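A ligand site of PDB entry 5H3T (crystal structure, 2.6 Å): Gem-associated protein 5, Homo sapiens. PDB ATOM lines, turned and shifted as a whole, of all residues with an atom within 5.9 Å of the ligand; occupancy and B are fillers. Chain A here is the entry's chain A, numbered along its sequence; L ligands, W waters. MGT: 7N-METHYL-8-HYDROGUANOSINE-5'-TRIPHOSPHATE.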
ATOM      1  N   TYR A 383       5.584   4.628 -13.084  1.00  0.00           N
ATOM      2  CA  TYR A 383       4.962   3.576 -13.876  1.00  0.00           C
ATOM      3  C   TYR A 383       3.747   2.941 -13.202  1.00  0.00           C
ATOM      4  O   TYR A 383       2.897   2.373 -13.906  1.00  0.00           O
ATOM      5  CB  TYR A 383       5.967   2.462 -14.174  1.00  0.00           C
ATOM      6  CG  TYR A 383       6.799   2.704 -15.400  1.00  0.00           C
ATOM      7  CD1 TYR A 383       6.220   2.678 -16.664  1.00  0.00           C
ATOM      8  CD2 TYR A 383       8.156   2.949 -15.313  1.00  0.00           C
ATOM      9  CE1 TYR A 383       6.993   2.905 -17.812  1.00  0.00           C
ATOM     10  CE2 TYR A 383       8.930   3.167 -16.438  1.00  0.00           C
ATOM     11  CZ  TYR A 383       8.347   3.148 -17.690  1.00  0.00           C
ATOM     12  OH  TYR A 383       9.142   3.369 -18.802  1.00  0.00           O
ATOM     13  N   THR A 430       8.160  -1.509 -13.287  1.00  0.00           N
ATOM     14  CA  THR A 430       7.040  -1.181 -14.143  1.00  0.00           C
ATOM     15  C   THR A 430       5.713  -1.814 -13.717  1.00  0.00           C
ATOM     16  O   THR A 430       4.716  -1.643 -14.405  1.00  0.00           O
ATOM     17  CB  THR A 430       7.364  -1.535 -15.592  1.00  0.00           C
ATOM     18  OG1 THR A 430       7.656  -2.937 -15.731  1.00  0.00           O
ATOM     19  CG2 THR A 430       8.521  -0.686 -16.064  1.00  0.00           C
ATOM     20  N   THR A 472       9.257  -6.796 -20.813  1.00  0.00           N
ATOM     21  CA  THR A 472       8.868  -6.046 -19.617  1.00  0.00           C
ATOM     22  C   THR A 472       7.712  -6.708 -18.865  1.00  0.00           C
ATOM     23  O   THR A 472       6.831  -7.334 -19.457  1.00  0.00           O
ATOM     24  CB  THR A 472       8.476  -4.623 -20.026  1.00  0.00           C
ATOM     25  OG1 THR A 472       9.584  -3.995 -20.660  1.00  0.00           O
ATOM     26  CG2 THR A 472       8.035  -3.780 -18.818  1.00  0.00           C
ATOM     27  N   TYR A 474       4.459  -6.023 -17.105  1.00  0.00           N
ATOM     28  CA  TYR A 474       3.421  -4.990 -17.101  1.00  0.00           C
ATOM     29  C   TYR A 474       2.285  -5.230 -16.106  1.00  0.00           C
ATOM     30  O   TYR A 474       1.652  -4.260 -15.684  1.00  0.00           O
ATOM     31  CB  TYR A 474       2.820  -4.855 -18.504  1.00  0.00           C
ATOM     32  CG  TYR A 474       3.754  -4.294 -19.544  1.00  0.00           C
ATOM     33  CD1 TYR A 474       4.048  -2.927 -19.583  1.00  0.00           C
ATOM     34  CD2 TYR A 474       4.300  -5.114 -20.537  1.00  0.00           C
ATOM     35  CE1 TYR A 474       4.876  -2.403 -20.537  1.00  0.00           C
ATOM     36  CE2 TYR A 474       5.143  -4.585 -21.507  1.00  0.00           C
ATOM     37  CZ  TYR A 474       5.424  -3.232 -21.508  1.00  0.00           C
ATOM     38  OH  TYR A 474       6.240  -2.679 -22.449  1.00  0.00           O
ATOM     39  N   THR A 475       1.987  -6.483 -15.744  1.00  0.00           N
ATOM     40  CA  THR A 475       0.875  -6.751 -14.835  1.00  0.00           C
ATOM     41  C   THR A 475       1.313  -7.698 -13.745  1.00  0.00           C
ATOM     42  O   THR A 475       2.079  -8.633 -13.985  1.00  0.00           O
ATOM     43  CB  THR A 475      -0.342  -7.376 -15.520  1.00  0.00           C
ATOM     44  OG1 THR A 475      -0.489  -6.873 -16.850  1.00  0.00           O
ATOM     45  CG2 THR A 475      -1.586  -7.037 -14.733  1.00  0.00           C
ATOM     46  N   GLY A 502       4.147 -10.663 -19.003  1.00  0.00           N
ATOM     47  CA  GLY A 502       5.252 -10.017 -19.700  1.00  0.00           C
ATOM     48  C   GLY A 502       4.888  -9.568 -21.096  1.00  0.00           C
ATOM     49  O   GLY A 502       3.933 -10.083 -21.676  1.00  0.00           O
ATOM     50  N   GLY A 503       5.635  -8.621 -21.666  1.00  0.00           N
ATOM     51  CA  GLY A 503       5.313  -8.097 -22.976  1.00  0.00           C
ATOM     52  C   GLY A 503       5.384  -9.123 -24.089  1.00  0.00           C
ATOM     53  O   GLY A 503       4.763  -8.936 -25.145  1.00  0.00           O
ATOM     54  N   THR A 540      -1.424  -9.802 -22.837  1.00  0.00           N
ATOM     55  CA  THR A 540      -0.828  -8.524 -22.483  1.00  0.00           C
ATOM     56  C   THR A 540      -1.341  -7.946 -21.167  1.00  0.00           C
ATOM     57  O   THR A 540      -0.733  -7.008 -20.652  1.00  0.00           O
ATOM     58  CB  THR A 540      -1.077  -7.491 -23.594  1.00  0.00           C
ATOM     59  OG1 THR A 540      -2.489  -7.348 -23.808  1.00  0.00           O
ATOM     60  CG2 THR A 540      -0.392  -7.924 -24.895  1.00  0.00           C
ATOM     61  N   GLU A 541      -2.402  -8.485 -20.608  1.00  0.00           N
ATOM     62  CA  GLU A 541      -2.953  -7.933 -19.383  1.00  0.00           C
ATOM     63  C   GLU A 541      -3.723  -9.029 -18.651  1.00  0.00           C
ATOM     64  O   GLU A 541      -4.434  -9.816 -19.282  1.00  0.00           O
ATOM     65  CB  GLU A 541      -3.863  -6.740 -19.713  1.00  0.00           C
ATOM     66  CG  GLU A 541      -4.783  -6.275 -18.579  1.00  0.00           C
ATOM     67  CD  GLU A 541      -4.049  -5.536 -17.458  1.00  0.00           C
ATOM     68  OE1 GLU A 541      -2.812  -5.386 -17.537  1.00  0.00           O
ATOM     69  OE2 GLU A 541      -4.724  -5.088 -16.498  1.00  0.00           O
ATOM     70  N   LEU A 580      -3.790  -3.652 -28.935  1.00  0.00           N
ATOM     71  CA  LEU A 580      -3.331  -4.245 -27.679  1.00  0.00           C
ATOM     72  C   LEU A 580      -4.085  -3.695 -26.470  1.00  0.00           C
ATOM     73  O   LEU A 580      -4.214  -2.472 -26.283  1.00  0.00           O
ATOM     74  CB  LEU A 580      -1.823  -3.968 -27.548  1.00  0.00           C
ATOM     75  CG  LEU A 580      -1.033  -4.504 -26.348  1.00  0.00           C
ATOM     76  CD1 LEU A 580       0.410  -4.802 -26.741  1.00  0.00           C
ATOM     77  CD2 LEU A 580      -1.079  -3.513 -25.205  1.00  0.00           C
ATOM     78  N   VAL A 581      -4.520  -4.600 -25.592  1.00  0.00           N
ATOM     79  CA  VAL A 581      -5.179  -4.226 -24.350  1.00  0.00           C
ATOM     80  C   VAL A 581      -4.134  -3.891 -23.298  1.00  0.00           C
ATOM     81  O   VAL A 581      -3.234  -4.694 -23.023  1.00  0.00           O
ATOM     82  CB  VAL A 581      -6.088  -5.352 -23.847  1.00  0.00           C
ATOM     83  CG1 VAL A 581      -6.820  -4.909 -22.584  1.00  0.00           C
ATOM     84  CG2 VAL A 581      -7.049  -5.797 -24.952  1.00  0.00           C
ATOM     85  N   ASN A 582      -4.281  -2.746 -22.641  1.00  0.00           N
ATOM     86  CA  ASN A 582      -3.300  -2.312 -21.652  1.00  0.00           C
ATOM     87  C   ASN A 582      -3.757  -2.524 -20.221  1.00  0.00           C
ATOM     88  O   ASN A 582      -2.918  -2.659 -19.320  1.00  0.00           O
ATOM     89  CB  ASN A 582      -2.960  -0.824 -21.829  1.00  0.00           C
ATOM     90  CG  ASN A 582      -2.219  -0.528 -23.132  1.00  0.00           C
ATOM     91  OD1 ASN A 582      -1.105  -1.025 -23.348  1.00  0.00           O
ATOM     92  ND2 ASN A 582      -2.812   0.290 -23.993  1.00  0.00           N
ATOM     93  N   THR A 583      -5.053  -2.508 -19.970  1.00  0.00           N
ATOM     94  CA  THR A 583      -5.516  -2.393 -18.595  1.00  0.00           C
ATOM     95  C   THR A 583      -6.906  -2.991 -18.554  1.00  0.00           C
ATOM     96  O   THR A 583      -7.719  -2.710 -19.441  1.00  0.00           O
ATOM     97  CB  THR A 583      -5.513  -0.933 -18.120  1.00  0.00           C
ATOM     98  OG1 THR A 583      -6.092  -0.840 -16.810  1.00  0.00           O
ATOM     99  CG2 THR A 583      -6.289  -0.039 -19.074  1.00  0.00           C
ATOM    100  N   ASN A 605      -4.714   0.370 -26.919  1.00  0.00           N
ATOM    101  CA  ASN A 605      -3.969   1.402 -27.602  1.00  0.00           C
ATOM    102  C   ASN A 605      -4.866   2.330 -28.399  1.00  0.00           C
ATOM    103  O   ASN A 605      -4.352   3.294 -28.981  1.00  0.00           O
ATOM    104  CB  ASN A 605      -2.918   0.800 -28.543  1.00  0.00           C
ATOM    105  CG  ASN A 605      -1.682   0.330 -27.814  1.00  0.00           C
ATOM    106  OD1 ASN A 605      -1.532   0.578 -26.610  1.00  0.00           O
ATOM    107  ND2 ASN A 605      -0.780  -0.338 -28.528  1.00  0.00           N
ATOM    108  N   LYS A 641      -3.968   6.549 -26.418  1.00  0.00           N
ATOM    109  CA  LYS A 641      -4.119   5.225 -25.814  1.00  0.00           C
ATOM    110  C   LYS A 641      -4.414   5.314 -24.321  1.00  0.00           C
ATOM    111  O   LYS A 641      -4.062   6.279 -23.633  1.00  0.00           O
ATOM    112  CB  LYS A 641      -2.872   4.377 -26.031  1.00  0.00           C
ATOM    113  CG  LYS A 641      -1.649   4.833 -25.283  1.00  0.00           C
ATOM    114  CD  LYS A 641      -0.436   4.028 -25.674  1.00  0.00           C
ATOM    115  CE  LYS A 641      -0.039   3.031 -24.599  1.00  0.00           C
ATOM    116  NZ  LYS A 641       1.199   2.279 -24.998  1.00  0.00           N
ATOM    117  N   THR A 643      -3.758   3.801 -20.702  1.00  0.00           N
ATOM    118  CA  THR A 643      -2.732   3.050 -19.984  1.00  0.00           C
ATOM    119  C   THR A 643      -3.243   2.432 -18.705  1.00  0.00           C
ATOM    120  O   THR A 643      -2.644   1.467 -18.214  1.00  0.00           O
ATOM    121  CB  THR A 643      -1.521   3.930 -19.636  1.00  0.00           C
ATOM    122  OG1 THR A 643      -1.925   5.035 -18.774  1.00  0.00           O
ATOM    123  CG2 THR A 643      -0.865   4.459 -20.876  1.00  0.00           C
ATOM    124  N   SER A 644      -4.324   2.956 -18.127  1.00  0.00           N
ATOM    125  CA  SER A 644      -4.779   2.486 -16.828  1.00  0.00           C
ATOM    126  C   SER A 644      -6.212   2.926 -16.613  1.00  0.00           C
ATOM    127  O   SER A 644      -6.608   4.008 -17.054  1.00  0.00           O
ATOM    128  CB  SER A 644      -3.869   3.025 -15.711  1.00  0.00           C
ATOM    129  OG  SER A 644      -4.093   2.355 -14.476  1.00  0.00           O
ATOM    130  N   TYR A 660      -2.587   8.616 -22.721  1.00  0.00           N
ATOM    131  CA  TYR A 660      -1.420   9.261 -23.305  1.00  0.00           C
ATOM    132  C   TYR A 660      -1.695  10.694 -23.719  1.00  0.00           C
ATOM    133  O   TYR A 660      -0.747  11.449 -23.940  1.00  0.00           O
ATOM    134  CB  TYR A 660      -0.912   8.455 -24.491  1.00  0.00           C
ATOM    135  CG  TYR A 660       0.278   7.596 -24.145  1.00  0.00           C
ATOM    136  CD1 TYR A 660       0.491   7.162 -22.837  1.00  0.00           C
ATOM    137  CD2 TYR A 660       1.206   7.223 -25.118  1.00  0.00           C
ATOM    138  CE1 TYR A 660       1.584   6.384 -22.510  1.00  0.00           C
ATOM    139  CE2 TYR A 660       2.287   6.440 -24.809  1.00  0.00           C
ATOM    140  CZ  TYR A 660       2.482   6.030 -23.496  1.00  0.00           C
ATOM    141  OH  TYR A 660       3.559   5.254 -23.175  1.00  0.00           O
ATOM    142  N   ARG A 684       2.684  12.125 -20.648  1.00  0.00           N
ATOM    143  CA  ARG A 684       1.776  10.995 -20.811  1.00  0.00           C
ATOM    144  C   ARG A 684       1.538  10.287 -19.480  1.00  0.00           C
ATOM    145  O   ARG A 684       2.494   9.921 -18.779  1.00  0.00           O
ATOM    146  CB  ARG A 684       2.339  10.015 -21.822  1.00  0.00           C
ATOM    147  CG  ARG A 684       2.623  10.566 -23.179  1.00  0.00           C
ATOM    148  CD  ARG A 684       3.748   9.761 -23.742  1.00  0.00           C
ATOM    149  NE  ARG A 684       3.739   9.647 -25.200  1.00  0.00           N
ATOM    150  CZ  ARG A 684       4.642   8.947 -25.869  1.00  0.00           C
ATOM    151  NH1 ARG A 684       5.616   8.323 -25.218  1.00  0.00           N
ATOM    152  NH2 ARG A 684       4.576   8.879 -27.200  1.00  0.00           N
ATOM    153  N   LEU A 686       0.508   7.182 -16.951  1.00  0.00           N
ATOM    154  CA  LEU A 686       0.783   5.761 -16.947  1.00  0.00           C
ATOM    155  C   LEU A 686      -0.037   4.982 -15.911  1.00  0.00           C
ATOM    156  O   LEU A 686      -0.188   3.773 -16.072  1.00  0.00           O
ATOM    157  CB  LEU A 686       2.289   5.510 -16.734  1.00  0.00           C
ATOM    158  CG  LEU A 686       3.233   6.322 -17.658  1.00  0.00           C
ATOM    159  CD1 LEU A 686       4.745   6.090 -17.403  1.00  0.00           C
ATOM    160  CD2 LEU A 686       2.905   6.073 -19.121  1.00  0.00           C
HETATM  161  PG  MGT L   1       4.956   3.453 -26.402  1.00  0.00           P
HETATM  162  O1G MGT L   1       5.126   2.634 -27.665  1.00  0.00           O
HETATM  163  O2G MGT L   1       3.577   4.037 -26.226  1.00  0.00           O
HETATM  164  O3G MGT L   1       6.088   4.413 -26.119  1.00  0.00           O
HETATM  165  O3B MGT L   1       5.073   2.359 -25.225  1.00  0.00           O
HETATM  166  PB  MGT L   1       5.802   0.952 -25.504  1.00  0.00           P
HETATM  167  O1B MGT L   1       4.925   0.133 -26.421  1.00  0.00           O
HETATM  168  O2B MGT L   1       7.236   1.236 -25.897  1.00  0.00           O
HETATM  169  O3A MGT L   1       5.800   0.258 -24.050  1.00  0.00           O
HETATM  170  PA  MGT L   1       6.285   1.086 -22.759  1.00  0.00           P
HETATM  171  O1A MGT L   1       7.341   0.272 -22.036  1.00  0.00           O
HETATM  172  O2A MGT L   1       6.587   2.499 -23.184  1.00  0.00           O
HETATM  173  O5' MGT L   1       4.965   1.101 -21.838  1.00  0.00           O
HETATM  174  C5' MGT L   1       4.540   2.307 -21.216  1.00  0.00           C
HETATM  175  C4' MGT L   1       3.097   2.171 -20.754  1.00  0.00           C
HETATM  176  O4' MGT L   1       2.306   1.566 -21.786  1.00  0.00           O
HETATM  177  C3' MGT L   1       2.988   1.283 -19.522  1.00  0.00           C
HETATM  178  O3' MGT L   1       2.783   2.090 -18.349  1.00  0.00           O
HETATM  179  C2' MGT L   1       1.854   0.309 -19.806  1.00  0.00           C
HETATM  180  O2' MGT L   1       0.664   0.592 -19.053  1.00  0.00           O
HETATM  181  C1' MGT L   1       1.541   0.460 -21.286  1.00  0.00           C
HETATM  182  N9  MGT L   1       1.854  -0.840 -21.970  1.00  0.00           N
HETATM  183  C8  MGT L   1       2.798  -0.729 -23.090  1.00  0.00           C
HETATM  184  N7  MGT L   1       2.802  -2.154 -23.431  1.00  0.00           N
HETATM  185  CM7 MGT L   1       3.684  -2.476 -24.578  1.00  0.00           C
HETATM  186  C5  MGT L   1       2.022  -2.926 -22.687  1.00  0.00           C
HETATM  187  C6  MGT L   1       1.738  -4.371 -22.691  1.00  0.00           C
HETATM  188  O6  MGT L   1       2.271  -5.148 -23.509  1.00  0.00           O
HETATM  189  N1  MGT L   1       0.884  -4.803 -21.758  1.00  0.00           N
HETATM  190  C2  MGT L   1       0.302  -3.973 -20.858  1.00  0.00           C
HETATM  191  N2  MGT L   1      -0.552  -4.518 -19.959  1.00  0.00           N
HETATM  192  N3  MGT L   1       0.524  -2.635 -20.798  1.00  0.00           N
HETATM  193  C4  MGT L   1       1.366  -2.059 -21.686  1.00  0.00           C
HETATM  194  O   HOH W   1      -1.415  -0.893 -17.955  1.00  0.00           O
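O1A of the ligand lies within hydrogen-bond range of OH of Tyr 474 (3.2 Å). The side-chain amino group (NZ) of Lys 641 lies within salt-bridge range of an oxygen (O2G) of the ligand, 3.2 Å away. The backbone carbonyl oxygen (O) of Asn 582 lies within hydrogen-bond range of a nitrogen (N2) of the ligand, at 3.1 Å. OH of Tyr 660 sits close to O2G of the ligand, at 3.3 Å. OE1 of Glu 541 lies within hydrogen-bond range of N2 of the ligand, 3.4 Å away. The backbone carbonyl oxygen (O) of Thr 540 sits at hydrogen-bond distance from a nitrogen (N2) of the ligand, 2.6 Å away. A nitrogen (N3) of the ligand sits close to the side-chain amide oxygen (OD1) of Asn 582, 3.4 Å away.
The side-chain hydroxyl of Thr 643 lies close to the backbone carbonyl oxygen of Leu 686, at 3.5 Å. The side-chain carboxylate of Glu 541 is in hydrogen-bond range of the side-chain hydroxyl of Thr 475 (2.8 Å). N of Tyr 660 is in hydrogen-bond range of O of Lys 641, at 2.9 Å. The side-chain amide nitrogen (ND2) of Asn 582 sits at hydrogen-bond distance from the side-chain amide oxygen (OD1) of Asn 605, 2.9 Å away. The side-chain hydroxyl (OG1) of Thr 540 sits at hydrogen-bond distance from the backbone carbonyl oxygen (O) of Val 581 (2.9 Å). The backbone carbonyl oxygen (O) of Leu 580 lies within hydrogen-bond range of the backbone NH (N) of Asn 605, 3.0 Å away.
CD1 of Tyr 383 touches O3' of the ligand, 3.9 Å away. Thr 475 touches the ligand (OG1 to N2, 3.9 Å). Leu 580 touches the ligand (CD1 to O6, 3.7 Å). O of Thr 643 touches O2' of the ligand (3.5 Å). CB of Leu 686 touches O3' of the ligand (3.8 Å).
Water W1 lies within hydrogen-bond range of the backbone carbonyl oxygen (O) of Thr 643 (2.7 Å), the backbone carbonyl oxygen (O) of Asn 582 (2.7 Å) and an oxygen (O2') of the ligand (2.8 Å).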
